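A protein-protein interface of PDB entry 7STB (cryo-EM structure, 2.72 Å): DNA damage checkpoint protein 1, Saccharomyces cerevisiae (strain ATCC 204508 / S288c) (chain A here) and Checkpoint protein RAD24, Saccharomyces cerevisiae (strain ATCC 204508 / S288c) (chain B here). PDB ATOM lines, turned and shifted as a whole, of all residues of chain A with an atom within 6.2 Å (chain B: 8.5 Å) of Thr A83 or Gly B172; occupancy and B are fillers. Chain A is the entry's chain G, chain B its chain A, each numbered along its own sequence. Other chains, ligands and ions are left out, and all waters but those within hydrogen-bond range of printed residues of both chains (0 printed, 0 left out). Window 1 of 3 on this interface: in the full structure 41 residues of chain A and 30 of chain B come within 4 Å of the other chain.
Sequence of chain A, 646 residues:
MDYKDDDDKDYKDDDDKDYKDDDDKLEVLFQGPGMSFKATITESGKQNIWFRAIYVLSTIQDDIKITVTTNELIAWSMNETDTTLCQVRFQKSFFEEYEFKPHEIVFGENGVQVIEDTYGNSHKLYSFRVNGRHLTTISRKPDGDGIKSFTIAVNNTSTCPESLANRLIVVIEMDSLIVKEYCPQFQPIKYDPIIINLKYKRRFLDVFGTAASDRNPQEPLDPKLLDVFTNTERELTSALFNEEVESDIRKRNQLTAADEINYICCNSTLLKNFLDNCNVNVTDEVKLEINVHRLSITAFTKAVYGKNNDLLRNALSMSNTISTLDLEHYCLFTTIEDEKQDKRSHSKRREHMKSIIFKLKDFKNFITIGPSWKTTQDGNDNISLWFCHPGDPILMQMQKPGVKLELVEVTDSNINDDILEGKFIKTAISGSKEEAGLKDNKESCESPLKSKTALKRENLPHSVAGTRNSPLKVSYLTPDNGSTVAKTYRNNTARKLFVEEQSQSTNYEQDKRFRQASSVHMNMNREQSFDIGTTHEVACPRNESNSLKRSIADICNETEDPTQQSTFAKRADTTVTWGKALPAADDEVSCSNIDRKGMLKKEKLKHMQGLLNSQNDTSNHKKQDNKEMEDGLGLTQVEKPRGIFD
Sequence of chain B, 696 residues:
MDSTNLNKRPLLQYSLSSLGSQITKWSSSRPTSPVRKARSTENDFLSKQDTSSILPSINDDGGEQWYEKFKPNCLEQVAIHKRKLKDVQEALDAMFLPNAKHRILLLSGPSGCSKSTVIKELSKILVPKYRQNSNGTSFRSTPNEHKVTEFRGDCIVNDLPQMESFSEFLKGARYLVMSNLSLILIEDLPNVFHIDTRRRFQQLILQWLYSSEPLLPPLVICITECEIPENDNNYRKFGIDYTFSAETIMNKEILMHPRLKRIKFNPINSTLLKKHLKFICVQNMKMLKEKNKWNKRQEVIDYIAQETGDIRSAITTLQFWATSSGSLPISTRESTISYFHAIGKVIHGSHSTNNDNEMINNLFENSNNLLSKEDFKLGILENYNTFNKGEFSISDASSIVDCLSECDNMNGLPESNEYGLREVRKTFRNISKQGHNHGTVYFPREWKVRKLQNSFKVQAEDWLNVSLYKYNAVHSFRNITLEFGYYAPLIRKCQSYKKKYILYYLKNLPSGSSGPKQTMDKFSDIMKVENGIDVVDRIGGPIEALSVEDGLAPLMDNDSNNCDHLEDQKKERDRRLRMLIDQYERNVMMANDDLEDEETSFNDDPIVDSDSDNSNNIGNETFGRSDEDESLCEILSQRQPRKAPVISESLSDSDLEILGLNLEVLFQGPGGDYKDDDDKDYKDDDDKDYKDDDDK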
ATOM      1  N   MET A  78     -34.114 -28.638 -21.220  1.00  0.00           N
ATOM      2  CA  MET A  78     -32.695 -28.323 -21.244  1.00  0.00           C
ATOM      3  C   MET A  78     -31.927 -29.633 -21.308  1.00  0.00           C
ATOM      4  O   MET A  78     -32.285 -30.598 -20.629  1.00  0.00           O
ATOM      5  CB  MET A  78     -32.282 -27.516 -20.007  1.00  0.00           C
ATOM      6  CG  MET A  78     -30.855 -26.999 -20.042  1.00  0.00           C
ATOM      7  SD  MET A  78     -30.424 -26.045 -18.575  1.00  0.00           S
ATOM      8  CE  MET A  78     -31.367 -24.548 -18.851  1.00  0.00           C
ATOM      9  N   ASN A  79     -30.878 -29.667 -22.124  1.00  0.00           N
ATOM     10  CA  ASN A  79     -30.120 -30.895 -22.300  1.00  0.00           C
ATOM     11  C   ASN A  79     -29.192 -31.132 -21.108  1.00  0.00           C
ATOM     12  O   ASN A  79     -29.011 -30.273 -20.241  1.00  0.00           O
ATOM     13  CB  ASN A  79     -29.316 -30.855 -23.601  1.00  0.00           C
ATOM     14  CG  ASN A  79     -28.374 -29.671 -23.674  1.00  0.00           C
ATOM     15  OD1 ASN A  79     -28.150 -28.973 -22.685  1.00  0.00           O
ATOM     16  ND2 ASN A  79     -27.812 -29.439 -24.854  1.00  0.00           N
ATOM     17  N   GLU A  80     -28.597 -32.326 -21.078  1.00  0.00           N
ATOM     18  CA  GLU A  80     -27.724 -32.692 -19.967  1.00  0.00           C
ATOM     19  C   GLU A  80     -26.507 -31.779 -19.893  1.00  0.00           C
ATOM     20  O   GLU A  80     -26.072 -31.400 -18.798  1.00  0.00           O
ATOM     21  CB  GLU A  80     -27.290 -34.151 -20.106  1.00  0.00           C
ATOM     22  CG  GLU A  80     -28.425 -35.150 -19.961  1.00  0.00           C
ATOM     23  CD  GLU A  80     -29.010 -35.170 -18.561  1.00  0.00           C
ATOM     24  OE1 GLU A  80     -28.255 -34.927 -17.597  1.00  0.00           O
ATOM     25  OE2 GLU A  80     -30.223 -35.427 -18.425  1.00  0.00           O
ATOM     26  N   THR A  81     -25.940 -31.416 -21.044  1.00  0.00           N
ATOM     27  CA  THR A  81     -24.752 -30.571 -21.067  1.00  0.00           C
ATOM     28  C   THR A  81     -25.039 -29.133 -20.659  1.00  0.00           C
ATOM     29  O   THR A  81     -24.092 -28.357 -20.497  1.00  0.00           O
ATOM     30  CB  THR A  81     -24.122 -30.587 -22.462  1.00  0.00           C
ATOM     31  OG1 THR A  81     -25.115 -30.277 -23.445  1.00  0.00           O
ATOM     32  CG2 THR A  81     -23.523 -31.950 -22.763  1.00  0.00           C
ATOM     33  N   ASP A  82     -26.307 -28.759 -20.491  1.00  0.00           N
ATOM     34  CA  ASP A  82     -26.686 -27.389 -20.145  1.00  0.00           C
ATOM     35  C   ASP A  82     -26.239 -26.402 -21.218  1.00  0.00           C
ATOM     36  O   ASP A  82     -25.915 -25.249 -20.924  1.00  0.00           O
ATOM     37  CB  ASP A  82     -26.121 -26.983 -18.780  1.00  0.00           C
ATOM     38  CG  ASP A  82     -26.891 -27.592 -17.627  1.00  0.00           C
ATOM     39  OD1 ASP A  82     -26.550 -28.721 -17.213  1.00  0.00           O
ATOM     40  OD2 ASP A  82     -27.835 -26.942 -17.132  1.00  0.00           O
ATOM     41  N   THR A  83     -26.221 -26.850 -22.473  1.00  0.00           N
ATOM     42  CA  THR A  83     -25.811 -26.010 -23.590  1.00  0.00           C
ATOM     43  C   THR A  83     -26.982 -25.455 -24.386  1.00  0.00           C
ATOM     44  O   THR A  83     -26.801 -24.474 -25.114  1.00  0.00           O
ATOM     45  CB  THR A  83     -24.897 -26.798 -24.538  1.00  0.00           C
ATOM     46  OG1 THR A  83     -25.492 -28.065 -24.842  1.00  0.00           O
ATOM     47  CG2 THR A  83     -23.535 -27.022 -23.902  1.00  0.00           C
ATOM     48  N   THR A  84     -28.168 -26.050 -24.269  1.00  0.00           N
ATOM     49  CA  THR A  84     -29.352 -25.587 -24.975  1.00  0.00           C
ATOM     50  C   THR A  84     -30.541 -25.563 -24.026  1.00  0.00           C
ATOM     51  O   THR A  84     -30.720 -26.474 -23.214  1.00  0.00           O
ATOM     52  CB  THR A  84     -29.670 -26.481 -26.184  1.00  0.00           C
ATOM     53  OG1 THR A  84     -30.585 -25.808 -27.054  1.00  0.00           O
ATOM     54  CG2 THR A  84     -30.282 -27.799 -25.732  1.00  0.00           C
ATOM     55  N   LEU A  85     -31.348 -24.510 -24.133  1.00  0.00           N
ATOM     56  CA  LEU A  85     -32.561 -24.365 -23.335  1.00  0.00           C
ATOM     57  C   LEU A  85     -33.684 -23.901 -24.248  1.00  0.00           C
ATOM     58  O   LEU A  85     -33.570 -22.851 -24.888  1.00  0.00           O
ATOM     59  CB  LEU A  85     -32.356 -23.372 -22.187  1.00  0.00           C
ATOM     60  N   LYS A 359     -24.443 -25.006 -32.350  1.00  0.00           N
ATOM     61  CA  LYS A 359     -24.994 -26.264 -32.828  1.00  0.00           C
ATOM     62  C   LYS A 359     -26.179 -26.014 -33.757  1.00  0.00           C
ATOM     63  O   LYS A 359     -26.838 -24.971 -33.705  1.00  0.00           O
ATOM     64  CB  LYS A 359     -25.415 -27.143 -31.648  1.00  0.00           C
ATOM     65  CG  LYS A 359     -25.874 -28.543 -32.043  1.00  0.00           C
ATOM     66  CD  LYS A 359     -26.274 -29.379 -30.836  1.00  0.00           C
ATOM     67  CE  LYS A 359     -25.073 -29.785 -29.998  1.00  0.00           C
ATOM     68  NZ  LYS A 359     -24.184 -30.730 -30.726  1.00  0.00           N
ATOM     69  N   VAL A 408     -32.110 -20.744 -26.251  1.00  0.00           N
ATOM     70  CA  VAL A 408     -30.813 -20.254 -25.802  1.00  0.00           C
ATOM     71  C   VAL A 408     -29.789 -21.343 -26.077  1.00  0.00           C
ATOM     72  O   VAL A 408     -30.016 -22.509 -25.737  1.00  0.00           O
ATOM     73  CB  VAL A 408     -30.826 -19.882 -24.307  1.00  0.00           C
ATOM     74  CG1 VAL A 408     -29.536 -19.175 -23.924  1.00  0.00           C
ATOM     75  CG2 VAL A 408     -32.028 -19.011 -23.980  1.00  0.00           C
ATOM     76  N   GLU A 409     -28.672 -20.970 -26.697  1.00  0.00           N
ATOM     77  CA  GLU A 409     -27.614 -21.924 -27.006  1.00  0.00           C
ATOM     78  C   GLU A 409     -26.260 -21.354 -26.613  1.00  0.00           C
ATOM     79  O   GLU A 409     -26.088 -20.143 -26.477  1.00  0.00           O
ATOM     80  CB  GLU A 409     -27.602 -22.305 -28.490  1.00  0.00           C
ATOM     81  CG  GLU A 409     -28.816 -23.097 -28.938  1.00  0.00           C
ATOM     82  CD  GLU A 409     -28.771 -23.437 -30.410  1.00  0.00           C
ATOM     83  OE1 GLU A 409     -27.857 -22.946 -31.100  1.00  0.00           O
ATOM     84  OE2 GLU A 409     -29.641 -24.201 -30.877  1.00  0.00           O
ATOM     85  N   VAL A 410     -25.298 -22.252 -26.418  1.00  0.00           N
ATOM     86  CA  VAL A 410     -23.936 -21.889 -26.048  1.00  0.00           C
ATOM     87  C   VAL A 410     -23.078 -21.905 -27.305  1.00  0.00           C
ATOM     88  O   VAL A 410     -23.069 -22.895 -28.048  1.00  0.00           O
ATOM     89  CB  VAL A 410     -23.376 -22.847 -24.982  1.00  0.00           C
ATOM     90  CG1 VAL A 410     -21.906 -22.566 -24.730  1.00  0.00           C
ATOM     91  CG2 VAL A 410     -24.173 -22.734 -23.694  1.00  0.00           C
ATOM     92  N   PHE B 139     -26.861 -18.505 -17.620  1.00  0.00           N
ATOM     93  CA  PHE B 139     -28.253 -18.834 -17.907  1.00  0.00           C
ATOM     94  C   PHE B 139     -29.193 -18.168 -16.908  1.00  0.00           C
ATOM     95  O   PHE B 139     -30.072 -17.384 -17.282  1.00  0.00           O
ATOM     96  CB  PHE B 139     -28.441 -20.353 -17.889  1.00  0.00           C
ATOM     97  CG  PHE B 139     -28.075 -21.026 -19.180  1.00  0.00           C
ATOM     98  CD1 PHE B 139     -26.768 -21.402 -19.436  1.00  0.00           C
ATOM     99  CD2 PHE B 139     -29.041 -21.287 -20.137  1.00  0.00           C
ATOM    100  CE1 PHE B 139     -26.432 -22.023 -20.623  1.00  0.00           C
ATOM    101  CE2 PHE B 139     -28.709 -21.908 -21.326  1.00  0.00           C
ATOM    102  CZ  PHE B 139     -27.405 -22.276 -21.569  1.00  0.00           C
ATOM    103  N   THR B 149     -20.044 -32.118 -15.380  1.00  0.00           N
ATOM    104  CA  THR B 149     -21.073 -32.494 -16.340  1.00  0.00           C
ATOM    105  C   THR B 149     -20.912 -33.977 -16.641  1.00  0.00           C
ATOM    106  O   THR B 149     -19.851 -34.404 -17.108  1.00  0.00           O
ATOM    107  CB  THR B 149     -20.965 -31.667 -17.623  1.00  0.00           C
ATOM    108  OG1 THR B 149     -21.220 -30.288 -17.329  1.00  0.00           O
ATOM    109  CG2 THR B 149     -21.963 -32.151 -18.662  1.00  0.00           C
ATOM    110  N   SER B 165     -26.702 -40.967 -29.095  1.00  0.00           N
ATOM    111  CA  SER B 165     -26.872 -40.197 -27.868  1.00  0.00           C
ATOM    112  C   SER B 165     -25.538 -39.652 -27.373  1.00  0.00           C
ATOM    113  O   SER B 165     -25.379 -38.440 -27.187  1.00  0.00           O
ATOM    114  CB  SER B 165     -27.530 -41.066 -26.796  1.00  0.00           C
ATOM    115  OG  SER B 165     -27.941 -40.286 -25.687  1.00  0.00           O
ATOM    116  N   PHE B 166     -24.547 -40.532 -27.203  1.00  0.00           N
ATOM    117  CA  PHE B 166     -23.268 -40.097 -26.650  1.00  0.00           C
ATOM    118  C   PHE B 166     -22.628 -39.034 -27.529  1.00  0.00           C
ATOM    119  O   PHE B 166     -22.101 -38.035 -27.025  1.00  0.00           O
ATOM    120  CB  PHE B 166     -22.329 -41.291 -26.484  1.00  0.00           C
ATOM    121  CG  PHE B 166     -21.016 -40.940 -25.844  1.00  0.00           C
ATOM    122  CD1 PHE B 166     -20.977 -40.290 -24.623  1.00  0.00           C
ATOM    123  CD2 PHE B 166     -19.820 -41.257 -26.466  1.00  0.00           C
ATOM    124  CE1 PHE B 166     -19.773 -39.964 -24.033  1.00  0.00           C
ATOM    125  CE2 PHE B 166     -18.612 -40.931 -25.880  1.00  0.00           C
ATOM    126  CZ  PHE B 166     -18.590 -40.285 -24.662  1.00  0.00           C
ATOM    127  N   SER B 167     -22.670 -39.227 -28.849  1.00  0.00           N
ATOM    128  CA  SER B 167     -22.183 -38.198 -29.758  1.00  0.00           C
ATOM    129  C   SER B 167     -22.822 -36.854 -29.440  1.00  0.00           C
ATOM    130  O   SER B 167     -22.125 -35.849 -29.253  1.00  0.00           O
ATOM    131  CB  SER B 167     -22.469 -38.605 -31.204  1.00  0.00           C
ATOM    132  OG  SER B 167     -22.064 -37.593 -32.108  1.00  0.00           O
ATOM    133  N   GLU B 168     -24.152 -36.826 -29.328  1.00  0.00           N
ATOM    134  CA  GLU B 168     -24.829 -35.567 -29.042  1.00  0.00           C
ATOM    135  C   GLU B 168     -24.357 -34.975 -27.723  1.00  0.00           C
ATOM    136  O   GLU B 168     -24.326 -33.749 -27.569  1.00  0.00           O
ATOM    137  CB  GLU B 168     -26.343 -35.769 -29.024  1.00  0.00           C
ATOM    138  CG  GLU B 168     -26.929 -36.140 -30.375  1.00  0.00           C
ATOM    139  CD  GLU B 168     -26.812 -35.020 -31.390  1.00  0.00           C
ATOM    140  OE1 GLU B 168     -26.860 -33.840 -30.985  1.00  0.00           O
ATOM    141  OE2 GLU B 168     -26.668 -35.321 -32.594  1.00  0.00           O
ATOM    142  N   PHE B 169     -23.989 -35.823 -26.762  1.00  0.00           N
ATOM    143  CA  PHE B 169     -23.395 -35.315 -25.532  1.00  0.00           C
ATOM    144  C   PHE B 169     -22.031 -34.696 -25.812  1.00  0.00           C
ATOM    145  O   PHE B 169     -21.774 -33.543 -25.444  1.00  0.00           O
ATOM    146  CB  PHE B 169     -23.279 -36.443 -24.504  1.00  0.00           C
ATOM    147  CG  PHE B 169     -22.671 -36.015 -23.198  1.00  0.00           C
ATOM    148  CD1 PHE B 169     -23.393 -35.247 -22.301  1.00  0.00           C
ATOM    149  CD2 PHE B 169     -21.377 -36.382 -22.868  1.00  0.00           C
ATOM    150  CE1 PHE B 169     -22.836 -34.852 -21.100  1.00  0.00           C
ATOM    151  CE2 PHE B 169     -20.815 -35.990 -21.671  1.00  0.00           C
ATOM    152  CZ  PHE B 169     -21.545 -35.225 -20.785  1.00  0.00           C
ATOM    153  N   LEU B 170     -21.160 -35.431 -26.507  1.00  0.00           N
ATOM    154  CA  LEU B 170     -19.802 -34.943 -26.718  1.00  0.00           C
ATOM    155  C   LEU B 170     -19.802 -33.647 -27.512  1.00  0.00           C
ATOM    156  O   LEU B 170     -19.107 -32.691 -27.151  1.00  0.00           O
ATOM    157  CB  LEU B 170     -18.961 -36.004 -27.427  1.00  0.00           C
ATOM    158  CG  LEU B 170     -18.421 -37.140 -26.556  1.00  0.00           C
ATOM    159  CD1 LEU B 170     -17.651 -38.129 -27.411  1.00  0.00           C
ATOM    160  CD2 LEU B 170     -17.542 -36.607 -25.431  1.00  0.00           C
ATOM    161  N   LYS B 171     -20.598 -33.582 -28.580  1.00  0.00           N
ATOM    162  CA  LYS B 171     -20.648 -32.370 -29.386  1.00  0.00           C
ATOM    163  C   LYS B 171     -21.129 -31.173 -28.582  1.00  0.00           C
ATOM    164  O   LYS B 171     -20.888 -30.031 -28.990  1.00  0.00           O
ATOM    165  CB  LYS B 171     -21.546 -32.586 -30.604  1.00  0.00           C
ATOM    166  CG  LYS B 171     -20.925 -33.476 -31.665  1.00  0.00           C
ATOM    167  CD  LYS B 171     -21.970 -34.032 -32.615  1.00  0.00           C
ATOM    168  CE  LYS B 171     -21.340 -34.913 -33.681  1.00  0.00           C
ATOM    169  NZ  LYS B 171     -20.463 -35.967 -33.100  1.00  0.00           N
ATOM    170  N   GLY B 172     -21.796 -31.400 -27.453  1.00  0.00           N
ATOM    171  CA  GLY B 172     -22.147 -30.310 -26.566  1.00  0.00           C
ATOM    172  C   GLY B 172     -21.045 -30.042 -25.563  1.00  0.00           C
ATOM    173  O   GLY B 172     -20.741 -28.888 -25.242  1.00  0.00           O
ATOM    174  N   ALA B 173     -20.422 -31.120 -25.078  1.00  0.00           N
ATOM    175  CA  ALA B 173     -19.395 -30.986 -24.052  1.00  0.00           C
ATOM    176  C   ALA B 173     -18.237 -30.114 -24.519  1.00  0.00           C
ATOM    177  O   ALA B 173     -17.592 -29.452 -23.699  1.00  0.00           O
ATOM    178  CB  ALA B 173     -18.886 -32.367 -23.641  1.00  0.00           C
ATOM    179  N   ARG B 174     -17.963 -30.091 -25.826  1.00  0.00           N
ATOM    180  CA  ARG B 174     -16.865 -29.272 -26.330  1.00  0.00           C
ATOM    181  C   ARG B 174     -17.070 -27.799 -26.008  1.00  0.00           C
ATOM    182  O   ARG B 174     -16.093 -27.051 -25.885  1.00  0.00           O
ATOM    183  CB  ARG B 174     -16.704 -29.452 -27.843  1.00  0.00           C
ATOM    184  CG  ARG B 174     -16.710 -30.892 -28.324  1.00  0.00           C
ATOM    185  CD  ARG B 174     -16.743 -30.976 -29.841  1.00  0.00           C
ATOM    186  NE  ARG B 174     -17.183 -32.287 -30.305  1.00  0.00           N
ATOM    187  CZ  ARG B 174     -16.432 -33.380 -30.286  1.00  0.00           C
ATOM    188  NH1 ARG B 174     -15.185 -33.356 -29.845  1.00  0.00           N
ATOM    189  NH2 ARG B 174     -16.946 -34.526 -30.723  1.00  0.00           N
ATOM    190  N   TYR B 175     -18.320 -27.362 -25.869  1.00  0.00           N
ATOM    191  CA  TYR B 175     -18.598 -25.947 -25.657  1.00  0.00           C
ATOM    192  C   TYR B 175     -18.420 -25.513 -24.208  1.00  0.00           C
ATOM    193  O   TYR B 175     -18.492 -24.312 -23.928  1.00  0.00           O
ATOM    194  CB  TYR B 175     -20.019 -25.625 -26.119  1.00  0.00           C
ATOM    195  CG  TYR B 175     -20.166 -25.577 -27.621  1.00  0.00           C
ATOM    196  CD1 TYR B 175     -20.469 -26.720 -28.344  1.00  0.00           C
ATOM    197  CD2 TYR B 175     -19.994 -24.387 -28.317  1.00  0.00           C
ATOM    198  CE1 TYR B 175     -20.601 -26.681 -29.717  1.00  0.00           C
ATOM    199  CE2 TYR B 175     -20.125 -24.339 -29.689  1.00  0.00           C
ATOM    200  CZ  TYR B 175     -20.428 -25.489 -30.384  1.00  0.00           C
ATOM    201  OH  TYR B 175     -20.559 -25.447 -31.751  1.00  0.00           O
ATOM    202  N   LEU B 176     -18.189 -26.447 -23.288  1.00  0.00           N
ATOM    203  CA  LEU B 176     -18.052 -26.122 -21.868  1.00  0.00           C
ATOM    204  C   LEU B 176     -16.587 -25.816 -21.554  1.00  0.00           C
ATOM    205  O   LEU B 176     -15.894 -26.550 -20.849  1.00  0.00           O
ATOM    206  CB  LEU B 176     -18.586 -27.263 -21.012  1.00  0.00           C
ATOM    207  CG  LEU B 176     -20.016 -27.705 -21.333  1.00  0.00           C
ATOM    208  CD1 LEU B 176     -20.401 -28.923 -20.510  1.00  0.00           C
ATOM    209  CD2 LEU B 176     -20.998 -26.566 -21.103  1.00  0.00           C
ATOM    210  N   VAL B 177     -16.122 -24.691 -22.101  1.00  0.00           N
ATOM    211  CA  VAL B 177     -14.748 -24.243 -21.931  1.00  0.00           C
ATOM    212  C   VAL B 177     -14.747 -22.755 -21.610  1.00  0.00           C
ATOM    213  O   VAL B 177     -15.717 -22.037 -21.866  1.00  0.00           O
ATOM    214  CB  VAL B 177     -13.883 -24.519 -23.179  1.00  0.00           C
ATOM    215  CG1 VAL B 177     -13.666 -26.012 -23.360  1.00  0.00           C
ATOM    216  CG2 VAL B 177     -14.523 -23.911 -24.420  1.00  0.00           C
ATOM    217  N   ASN B 180     -17.571 -21.004 -19.744  1.00  0.00           N
ATOM    218  CA  ASN B 180     -18.440 -22.139 -19.462  1.00  0.00           C
ATOM    219  C   ASN B 180     -17.647 -23.382 -19.082  1.00  0.00           C
ATOM    220  O   ASN B 180     -18.080 -24.505 -19.358  1.00  0.00           O
ATOM    221  CB  ASN B 180     -19.334 -22.430 -20.668  1.00  0.00           C
ATOM    222  CG  ASN B 180     -19.930 -21.175 -21.271  1.00  0.00           C
ATOM    223  OD1 ASN B 180     -19.564 -20.768 -22.372  1.00  0.00           O
ATOM    224  ND2 ASN B 180     -20.854 -20.554 -20.548  1.00  0.00           N
ATOM    225  N   ILE B 184     -15.784 -32.676 -17.646  1.00  0.00           N
ATOM    226  CA  ILE B 184     -16.621 -33.680 -18.292  1.00  0.00           C
ATOM    227  C   ILE B 184     -16.272 -35.035 -17.689  1.00  0.00           C
ATOM    228  O   ILE B 184     -15.164 -35.542 -17.879  1.00  0.00           O
ATOM    229  CB  ILE B 184     -16.428 -33.679 -19.813  1.00  0.00           C
ATOM    230  CG1 ILE B 184     -16.522 -32.255 -20.369  1.00  0.00           C
ATOM    231  CG2 ILE B 184     -17.451 -34.585 -20.483  1.00  0.00           C
ATOM    232  CD1 ILE B 184     -17.800 -31.532 -20.012  1.00  0.00           C
ATOM    233  N   TRP B 208     -12.111 -37.156 -30.363  1.00  0.00           N
ATOM    234  CA  TRP B 208     -11.803 -36.201 -29.303  1.00  0.00           C
ATOM    235  C   TRP B 208     -10.299 -36.087 -29.093  1.00  0.00           C
ATOM    236  O   TRP B 208      -9.763 -34.980 -28.962  1.00  0.00           O
ATOM    237  CB  TRP B 208     -12.494 -36.620 -28.004  1.00  0.00           C
ATOM    238  CG  TRP B 208     -12.363 -35.613 -26.899  1.00  0.00           C
ATOM    239  CD1 TRP B 208     -11.280 -35.414 -26.095  1.00  0.00           C
ATOM    240  CD2 TRP B 208     -13.354 -34.667 -26.477  1.00  0.00           C
ATOM    241  NE1 TRP B 208     -11.532 -34.404 -25.201  1.00  0.00           N
ATOM    242  CE2 TRP B 208     -12.798 -33.928 -25.414  1.00  0.00           C
ATOM    243  CE3 TRP B 208     -14.654 -34.374 -26.895  1.00  0.00           C
ATOM    244  CZ2 TRP B 208     -13.499 -32.916 -24.764  1.00  0.00           C
ATOM    245  CZ3 TRP B 208     -15.347 -33.369 -26.248  1.00  0.00           C
ATOM    246  CH2 TRP B 208     -14.768 -32.651 -25.195  1.00  0.00           C
ATOM    247  N   PRO B 217     -12.334 -28.948 -23.072  1.00  0.00           N
ATOM    248  CA  PRO B 217     -12.461 -29.111 -21.624  1.00  0.00           C
ATOM    249  C   PRO B 217     -11.814 -30.405 -21.168  1.00  0.00           C
ATOM    250  O   PRO B 217     -11.713 -31.363 -21.951  1.00  0.00           O
ATOM    251  CB  PRO B 217     -13.979 -29.139 -21.410  1.00  0.00           C
ATOM    252  CG  PRO B 217     -14.501 -29.755 -22.656  1.00  0.00           C
ATOM    253  CD  PRO B 217     -13.569 -29.340 -23.775  1.00  0.00           C
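OG of Ser B167 sits at hydrogen-bond distance from NZ of Lys B171, 2.5 Å away. ND2 of Asn A79 is in hydrogen-bond range of OG1 of Thr A81. The backbone NH (N) of Asp A82 sits at hydrogen-bond distance from the side-chain amide oxygen (OD1) of Asn A79 (2.9 Å). The side-chain amide nitrogen (ND2) of Asn A79 sits at hydrogen-bond distance from the side-chain hydroxyl (OG1) of Thr A83 (2.7 Å). The side-chain hydroxyl of Thr A81 lies within hydrogen-bond range of the side-chain hydroxyl of Thr A83 (2.6 Å). The backbone carbonyl oxygen of Thr A83 is in hydrogen-bond range of the backbone NH of Val A410 (3.0 Å).
Of the 12 printed residues of chain A, 6 touch a printed residue of chain B. Printed residues of chain A that touch a printed residue of chain B: Thr A81, Asp A82, Thr A83, Lys A359, Val A408 and Val A410. Hydrophobic or aromatic side chains of chain A within 4 Å of the printed part of chain B: Val A408 and Val A410. Among the printed residues, 12 pairs touch across the chains.
Among the printed residues, pairs that only touch across the chains: Lys A359 with Lys B171 (3.2 Å), Asp A82 with Phe B139 (3.3 Å), Thr A81 with Phe B169 (3.3 Å), Val A410 with Tyr B175 (3.4 Å), Thr A83 with Gly B172 (3.6 Å), Thr A81 with Leu B176 (3.6 Å), Val A410 with Asn B180 (3.8 Å), Thr A83 with Leu B176 (3.8 Å), Val A408 with Phe B139 (3.9 Å), Val A410 with Phe B139 (3.9 Å), Lys A359 with Tyr B175 (3.95 Å) and Thr A81 with Ala B173 (3.96 Å).
Thr A83 touches two residues of chain B. Gly B172 touches one residue of chain A. Of the printed residues of chain A, Phe B169 touches Thr A81. Printed residues of chain A within 4 Å of Lys B171: Lys A359. Printed residues of chain B within 4 Å of Thr A81: Phe B169, Ala B173 and Leu B176. Of the printed residues of chain B, Val A408 touches Phe B139. Printed residues of chain B within 4 Å of Val A410: Phe B139 (3.9 Å), Tyr B175 (3.4 Å) and Asn B180 (3.8 Å). Asn A79 touches none of the printed residues of chain B. The nearest residue of chain B that does not touch Thr A83 is Phe B139 (4.2 Å). The nearest printed residue of chain B that does not touch Thr A81 is Thr B149 (4.01 Å).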
